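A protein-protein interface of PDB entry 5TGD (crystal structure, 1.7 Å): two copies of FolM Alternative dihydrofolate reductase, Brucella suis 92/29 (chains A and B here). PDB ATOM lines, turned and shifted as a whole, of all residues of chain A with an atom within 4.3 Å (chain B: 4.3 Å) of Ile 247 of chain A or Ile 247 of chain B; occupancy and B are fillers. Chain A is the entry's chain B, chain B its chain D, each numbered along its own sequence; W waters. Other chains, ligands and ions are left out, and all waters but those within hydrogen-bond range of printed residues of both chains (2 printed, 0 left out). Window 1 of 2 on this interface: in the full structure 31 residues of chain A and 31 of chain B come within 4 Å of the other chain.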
ATOM      1  N   ALA A 194      14.465  15.301  14.370  1.00  0.00           N
ATOM      2  CA  ALA A 194      14.844  15.631  13.006  1.00  0.00           C
ATOM      3  C   ALA A 194      16.338  15.899  12.915  1.00  0.00           C
ATOM      4  O   ALA A 194      17.003  16.202  13.910  1.00  0.00           O
ATOM      5  CB  ALA A 194      14.050  16.839  12.477  1.00  0.00           C
ATOM      6  N   ILE A 195      16.853  15.764  11.693  1.00  0.00           N
ATOM      7  CA  ILE A 195      18.211  16.150  11.327  1.00  0.00           C
ATOM      8  C   ILE A 195      18.113  17.133  10.169  1.00  0.00           C
ATOM      9  O   ILE A 195      17.400  16.878   9.191  1.00  0.00           O
ATOM     10  CB  ILE A 195      19.071  14.937  10.925  1.00  0.00           C
ATOM     11  CG1 ILE A 195      19.167  13.926  12.067  1.00  0.00           C
ATOM     12  CG2 ILE A 195      20.457  15.400  10.489  1.00  0.00           C
ATOM     13  CD1 ILE A 195      19.886  12.626  11.676  1.00  0.00           C
ATOM     14  N   ALA A 196      18.817  18.259  10.280  1.00  0.00           N
ATOM     15  CA  ALA A 196      18.830  19.286   9.241  1.00  0.00           C
ATOM     16  C   ALA A 196      20.217  19.303   8.617  1.00  0.00           C
ATOM     17  O   ALA A 196      21.128  19.970   9.130  1.00  0.00           O
ATOM     18  CB  ALA A 196      18.478  20.656   9.824  1.00  0.00           C
ATOM     19  N   TYR A 235      21.825   8.626  18.626  1.00  0.00           N
ATOM     20  CA  TYR A 235      21.709   9.526  19.769  1.00  0.00           C
ATOM     21  C   TYR A 235      20.242   9.757  20.139  1.00  0.00           C
ATOM     22  O   TYR A 235      19.864   9.654  21.313  1.00  0.00           O
ATOM     23  CB  TYR A 235      22.414  10.857  19.477  1.00  0.00           C
ATOM     24  CG  TYR A 235      22.078  11.920  20.495  1.00  0.00           C
ATOM     25  CD1 TYR A 235      22.605  11.862  21.780  1.00  0.00           C
ATOM     26  CD2 TYR A 235      21.215  12.966  20.182  1.00  0.00           C
ATOM     27  CE1 TYR A 235      22.298  12.808  22.720  1.00  0.00           C
ATOM     28  CE2 TYR A 235      20.899  13.920  21.124  1.00  0.00           C
ATOM     29  CZ  TYR A 235      21.440  13.834  22.388  1.00  0.00           C
ATOM     30  OH  TYR A 235      21.127  14.780  23.337  1.00  0.00           O
ATOM     31  N   PHE A 236      19.401  10.070  19.147  1.00  0.00           N
ATOM     32  CA  PHE A 236      17.974  10.232  19.421  1.00  0.00           C
ATOM     33  C   PHE A 236      17.373   8.955  20.008  1.00  0.00           C
ATOM     34  O   PHE A 236      16.554   9.011  20.933  1.00  0.00           O
ATOM     35  CB  PHE A 236      17.224  10.631  18.143  1.00  0.00           C
ATOM     36  CG  PHE A 236      17.409  12.076  17.735  1.00  0.00           C
ATOM     37  CD1 PHE A 236      17.471  13.088  18.687  1.00  0.00           C
ATOM     38  CD2 PHE A 236      17.503  12.423  16.391  1.00  0.00           C
ATOM     39  CE1 PHE A 236      17.630  14.421  18.304  1.00  0.00           C
ATOM     40  CE2 PHE A 236      17.668  13.762  16.002  1.00  0.00           C
ATOM     41  CZ  PHE A 236      17.736  14.757  16.961  1.00  0.00           C
ATOM     42  N   ILE A 242      14.015  13.134  24.616  1.00  0.00           N
ATOM     43  CA  ILE A 242      14.100  14.088  23.510  1.00  0.00           C
ATOM     44  C   ILE A 242      12.951  13.844  22.537  1.00  0.00           C
ATOM     45  O   ILE A 242      12.820  12.748  21.977  1.00  0.00           O
ATOM     46  CB  ILE A 242      15.444  13.967  22.773  1.00  0.00           C
ATOM     47  CG1 ILE A 242      16.630  14.074  23.726  1.00  0.00           C
ATOM     48  CG2 ILE A 242      15.535  15.004  21.660  1.00  0.00           C
ATOM     49  CD1 ILE A 242      17.928  13.734  23.046  1.00  0.00           C
ATOM     50  N   GLN A 245      12.474  17.808  18.357  1.00  0.00           N
ATOM     51  CA  GLN A 245      13.674  18.618  18.221  1.00  0.00           C
ATOM     52  C   GLN A 245      14.515  18.168  17.030  1.00  0.00           C
ATOM     53  O   GLN A 245      14.348  17.072  16.489  1.00  0.00           O
ATOM     54  CB  GLN A 245      14.515  18.579  19.507  1.00  0.00           C
ATOM     55  CG  GLN A 245      13.730  19.024  20.739  1.00  0.00           C
ATOM     56  CD  GLN A 245      14.474  18.744  22.031  1.00  0.00           C
ATOM     57  OE1 GLN A 245      15.648  19.098  22.171  1.00  0.00           O
ATOM     58  NE2 GLN A 245      13.798  18.099  22.982  1.00  0.00           N
ATOM     59  N   MET A 246      15.453  19.039  16.655  1.00  0.00           N
ATOM     60  CA  MET A 246      16.243  18.883  15.448  1.00  0.00           C
ATOM     61  C   MET A 246      17.686  19.264  15.735  1.00  0.00           C
ATOM     62  O   MET A 246      17.951  20.233  16.455  1.00  0.00           O
ATOM     63  CB  MET A 246      15.676  19.765  14.324  1.00  0.00           C
ATOM     64  CG  MET A 246      16.383  19.636  12.994  1.00  0.00           C
ATOM     65  SD  MET A 246      15.368  20.305  11.672  1.00  0.00           S
ATOM     66  CE  MET A 246      15.286  22.035  12.166  1.00  0.00           C
ATOM     67  N   ILE A 247      18.614  18.501  15.170  1.00  0.00           N
ATOM     68  CA  ILE A 247      20.027  18.855  15.146  1.00  0.00           C
ATOM     69  C   ILE A 247      20.384  19.189  13.705  1.00  0.00           C
ATOM     70  O   ILE A 247      20.078  18.412  12.789  1.00  0.00           O
ATOM     71  CB  ILE A 247      20.908  17.710  15.678  1.00  0.00           C
ATOM     72  CG1 ILE A 247      20.757  17.572  17.191  1.00  0.00           C
ATOM     73  CG2 ILE A 247      22.370  17.962  15.344  1.00  0.00           C
ATOM     74  CD1 ILE A 247      21.430  18.701  17.954  1.00  0.00           C
ATOM     75  N   ALA A 248      21.020  20.342  13.498  1.00  0.00           N
ATOM     76  CA  ALA A 248      21.510  20.723  12.177  1.00  0.00           C
ATOM     77  C   ALA A 248      22.963  20.281  12.068  1.00  0.00           C
ATOM     78  O   ALA A 248      23.839  20.835  12.729  1.00  0.00           O
ATOM     79  CB  ALA A 248      21.364  22.226  11.943  1.00  0.00           C
ATOM     80  N   LEU A 249      23.216  19.261  11.252  1.00  0.00           N
ATOM     81  CA  LEU A 249      24.581  18.830  10.958  1.00  0.00           C
ATOM     82  C   LEU A 249      25.036  19.646   9.756  1.00  0.00           C
ATOM     83  O   LEU A 249      25.013  19.183   8.612  1.00  0.00           O
ATOM     84  CB  LEU A 249      24.623  17.335  10.671  1.00  0.00           C
ATOM     85  CG  LEU A 249      24.149  16.387  11.774  1.00  0.00           C
ATOM     86  CD1 LEU A 249      24.064  14.948  11.226  1.00  0.00           C
ATOM     87  CD2 LEU A 249      25.062  16.457  13.003  1.00  0.00           C
ATOM     88  N   ALA B 194      24.343  23.552  23.800  1.00  0.00           N
ATOM     89  CA  ALA B 194      23.645  23.718  25.067  1.00  0.00           C
ATOM     90  C   ALA B 194      22.735  22.528  25.329  1.00  0.00           C
ATOM     91  O   ALA B 194      22.338  21.799  24.412  1.00  0.00           O
ATOM     92  CB  ALA B 194      22.837  25.027  25.088  1.00  0.00           C
ATOM     93  N   ILE B 195      22.431  22.340  26.611  1.00  0.00           N
ATOM     94  CA  ILE B 195      21.432  21.384  27.077  1.00  0.00           C
ATOM     95  C   ILE B 195      20.401  22.170  27.871  1.00  0.00           C
ATOM     96  O   ILE B 195      20.765  23.000  28.712  1.00  0.00           O
ATOM     97  CB  ILE B 195      22.056  20.280  27.948  1.00  0.00           C
ATOM     98  CG1 ILE B 195      23.137  19.527  27.159  1.00  0.00           C
ATOM     99  CG2 ILE B 195      20.966  19.331  28.465  1.00  0.00           C
ATOM    100  CD1 ILE B 195      23.962  18.504  27.990  1.00  0.00           C
ATOM    101  N   ALA B 196      19.121  21.926  27.592  1.00  0.00           N
ATOM    102  CA  ALA B 196      18.028  22.572  28.313  1.00  0.00           C
ATOM    103  C   ALA B 196      17.336  21.516  29.164  1.00  0.00           C
ATOM    104  O   ALA B 196      16.444  20.803  28.679  1.00  0.00           O
ATOM    105  CB  ALA B 196      17.041  23.228  27.343  1.00  0.00           C
ATOM    106  N   TYR B 235      27.984  13.407  22.812  1.00  0.00           N
ATOM    107  CA  TYR B 235      27.409  13.519  21.477  1.00  0.00           C
ATOM    108  C   TYR B 235      27.847  14.819  20.801  1.00  0.00           C
ATOM    109  O   TYR B 235      28.263  14.823  19.636  1.00  0.00           O
ATOM    110  CB  TYR B 235      25.881  13.430  21.556  1.00  0.00           C
ATOM    111  CG  TYR B 235      25.235  13.823  20.253  1.00  0.00           C
ATOM    112  CD1 TYR B 235      25.316  12.991  19.134  1.00  0.00           C
ATOM    113  CD2 TYR B 235      24.577  15.042  20.124  1.00  0.00           C
ATOM    114  CE1 TYR B 235      24.744  13.376  17.922  1.00  0.00           C
ATOM    115  CE2 TYR B 235      24.008  15.419  18.937  1.00  0.00           C
ATOM    116  CZ  TYR B 235      24.103  14.592  17.839  1.00  0.00           C
ATOM    117  OH  TYR B 235      23.536  15.003  16.659  1.00  0.00           O
ATOM    118  N   PHE B 236      27.771  15.937  21.529  1.00  0.00           N
ATOM    119  CA  PHE B 236      28.250  17.207  20.989  1.00  0.00           C
ATOM    120  C   PHE B 236      29.743  17.148  20.677  1.00  0.00           C
ATOM    121  O   PHE B 236      30.193  17.673  19.655  1.00  0.00           O
ATOM    122  CB  PHE B 236      27.964  18.346  21.979  1.00  0.00           C
ATOM    123  CG  PHE B 236      26.528  18.816  21.996  1.00  0.00           C
ATOM    124  CD1 PHE B 236      25.786  18.896  20.822  1.00  0.00           C
ATOM    125  CD2 PHE B 236      25.924  19.181  23.191  1.00  0.00           C
ATOM    126  CE1 PHE B 236      24.453  19.346  20.834  1.00  0.00           C
ATOM    127  CE2 PHE B 236      24.594  19.635  23.215  1.00  0.00           C
ATOM    128  CZ  PHE B 236      23.857  19.709  22.031  1.00  0.00           C
ATOM    129  N   ILE B 242      28.301  20.381  14.611  1.00  0.00           N
ATOM    130  CA  ILE B 242      27.228  20.974  15.403  1.00  0.00           C
ATOM    131  C   ILE B 242      27.775  22.155  16.196  1.00  0.00           C
ATOM    132  O   ILE B 242      28.686  21.994  17.023  1.00  0.00           O
ATOM    133  CB  ILE B 242      26.598  19.940  16.347  1.00  0.00           C
ATOM    134  CG1 ILE B 242      26.143  18.712  15.569  1.00  0.00           C
ATOM    135  CG2 ILE B 242      25.431  20.539  17.112  1.00  0.00           C
ATOM    136  CD1 ILE B 242      25.827  17.535  16.466  1.00  0.00           C
ATOM    137  N   GLN B 245      23.655  25.184  19.030  1.00  0.00           N
ATOM    138  CA  GLN B 245      22.394  24.468  19.130  1.00  0.00           C
ATOM    139  C   GLN B 245      22.197  23.899  20.523  1.00  0.00           C
ATOM    140  O   GLN B 245      23.133  23.797  21.328  1.00  0.00           O
ATOM    141  CB  GLN B 245      22.317  23.361  18.081  1.00  0.00           C
ATOM    142  CG  GLN B 245      22.419  23.912  16.665  1.00  0.00           C
ATOM    143  CD  GLN B 245      22.538  22.819  15.643  1.00  0.00           C
ATOM    144  OE1 GLN B 245      21.695  21.931  15.578  1.00  0.00           O
ATOM    145  NE2 GLN B 245      23.594  22.874  14.830  1.00  0.00           N
ATOM    146  N   MET B 246      20.948  23.511  20.786  1.00  0.00           N
ATOM    147  CA  MET B 246      20.534  23.057  22.106  1.00  0.00           C
ATOM    148  C   MET B 246      19.688  21.802  21.981  1.00  0.00           C
ATOM    149  O   MET B 246      18.926  21.654  21.022  1.00  0.00           O
ATOM    150  CB  MET B 246      19.739  24.151  22.834  1.00  0.00           C
ATOM    151  CG  MET B 246      19.401  23.834  24.281  1.00  0.00           C
ATOM    152  SD  MET B 246      19.038  25.349  25.193  1.00  0.00           S
ATOM    153  CE  MET B 246      17.584  25.952  24.343  1.00  0.00           C
ATOM    154  N   ILE B 247      19.845  20.900  22.943  1.00  0.00           N
ATOM    155  CA  ILE B 247      18.953  19.762  23.138  1.00  0.00           C
ATOM    156  C   ILE B 247      18.243  19.951  24.471  1.00  0.00           C
ATOM    157  O   ILE B 247      18.893  20.166  25.505  1.00  0.00           O
ATOM    158  CB  ILE B 247      19.717  18.421  23.119  1.00  0.00           C
ATOM    159  CG1 ILE B 247      20.236  18.113  21.719  1.00  0.00           C
ATOM    160  CG2 ILE B 247      18.831  17.277  23.630  1.00  0.00           C
ATOM    161  CD1 ILE B 247      19.130  17.710  20.736  1.00  0.00           C
ATOM    162  N   ALA B 248      16.915  19.861  24.453  1.00  0.00           N
ATOM    163  CA  ALA B 248      16.128  19.881  25.685  1.00  0.00           C
ATOM    164  C   ALA B 248      15.939  18.442  26.157  1.00  0.00           C
ATOM    165  O   ALA B 248      15.215  17.663  25.531  1.00  0.00           O
ATOM    166  CB  ALA B 248      14.787  20.581  25.469  1.00  0.00           C
ATOM    167  N   LEU B 249      16.616  18.075  27.246  1.00  0.00           N
ATOM    168  CA  LEU B 249      16.375  16.792  27.907  1.00  0.00           C
ATOM    169  C   LEU B 249      15.262  17.037  28.918  1.00  0.00           C
ATOM    170  O   LEU B 249      15.493  17.240  30.111  1.00  0.00           O
ATOM    171  CB  LEU B 249      17.647  16.271  28.571  1.00  0.00           C
ATOM    172  CG  LEU B 249      18.851  16.147  27.648  1.00  0.00           C
ATOM    173  CD1 LEU B 249      20.101  15.798  28.453  1.00  0.00           C
ATOM    174  CD2 LEU B 249      18.569  15.096  26.606  1.00  0.00           C
HETATM  175  O   HOH W   1      17.765  21.935  18.598  1.00  0.00           O
HETATM  176  O   HOH W   2      12.048  16.673  24.614  1.00  0.00           O
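The side-chain amide oxygen (OE1) of Gln 245 of chain A sits at hydrogen-bond distance from the backbone NH (N) of Ala 248 of chain B (2.7 Å). N of Ala 248 of chain A sits at hydrogen-bond distance from OE1 of Gln 245 of chain B (2.7 Å).
Tyr 235 of chain B touches Tyr 235 of chain A (CD1 to CB, 3.6 Å). Ile 247 of chain B touches Tyr 235 of chain A. Ile 247 of chain B touches Ile 242 of chain A (CG2 to CD1, 3.7 Å). CD2 of Leu 249 of chain B touches CG1 of Ile 242 of chain A, 3.6 Å away. Gln 245 of chain A touches Ile 247 of chain B. Ile 247 of chain A touches Tyr 235 of chain B (CG2 to OH, 3.4 Å). Ile 247 of chain A touches Ile 242 of chain B. Gln 245 of chain B touches Ile 247 of chain A. Ile 247 of chain B touches Ile 247 of chain A. Ile 242 of chain B touches Leu 249 of chain A (CG1 to CD2, 3.6 Å).
Of the printed residues of chain B, Tyr 235 of chain A touches Tyr 235 (3.6 Å) and Ile 247 (3.4 Å). Phe 236 of chain A touches none of the printed residues of chain B. Printed residues of chain B within 4 Å of Ile 242 of chain A: Ile 247 (3.7 Å) and Leu 249 (3.6 Å). Of the printed residues of chain B, Gln 245 of chain A touches Ile 247 and Ala 248. Ile 247 of chain A touches four residues of chain B. Printed residues of chain A within 4 Å of Tyr 235 of chain B: Tyr 235 and Ile 247. Ile 247 of chain B touches just these residues of chain A: Tyr 235, Ile 242, Gln 245 and Ile 247. Printed residues of chain A within 4 Å of Ala 248 of chain B: Gln 245. The nearest printed residue of chain A that does not touch Ile 247 of chain B is Phe 236 of chain A (4.4 Å).
The backbone NH (N) of Ile 247 of chain A is in hydrogen-bond range of the backbone carbonyl oxygen (O) of Ala 194 of chain A. The backbone carbonyl oxygen of Gln 245 of chain B sits at hydrogen-bond distance from the backbone NH of Ala 194 of chain B (2.8 Å). The backbone NH (N) of Ala 196 of chain A sits at hydrogen-bond distance from the backbone carbonyl oxygen (O) of Ile 247 of chain A (2.8 Å). The backbone carbonyl oxygen (O) of Ala 196 of chain B lies within hydrogen-bond range of the backbone NH (N) of Leu 249 of chain B, 3.1 Å away. N of Ala 194 of chain A sits at hydrogen-bond distance from O of Gln 245 of chain A, at 2.8 Å. The backbone NH of Ala 196 of chain B is in hydrogen-bond range of the backbone carbonyl oxygen of Ile 247 of chain B (2.7 Å).
Tyr 235 of chain B touches its own counterpart, Tyr 235 of chain A. Gln 245 of chain A touches Ile 247 of chain B, and with the chains exchanged Ile 247 of chain A touches Gln 245 of chain B. Gln 245 of chain A touches Ala 248 of chain B, and with the chains exchanged Ala 248 of chain A touches Gln 245 of chain B. Ile 247 of chain A touches its own counterpart, Ile 247 of chain B. Of the 12 pairs that touch across the chains among the printed residues, 12 have their exchanged pair printed and touching as well.
Water W1 bridges the backbone carbonyl oxygen of Met 246 of chain B (2.7 Å) and the backbone carbonyl oxygen of Met 246 of chain A (2.7 Å). Water W2 bridges the side-chain amide nitrogen of Gln 245 of chain A (2.8 Å) and the backbone carbonyl oxygen of Ala 248 of chain B (3.4 Å).
Hydrophobic or aromatic side chains of chain B that line the printed part of chain A: Tyr 235, Ile 242, Ile 247, Ala 248 and Leu 249. Of the 11 printed residues of chain A, 6 touch a printed residue of chain B. Among the printed residues, no Asp or Glu carboxylate lies within 4 Å of a Lys or Arg side-chain nitrogen of the other chain.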
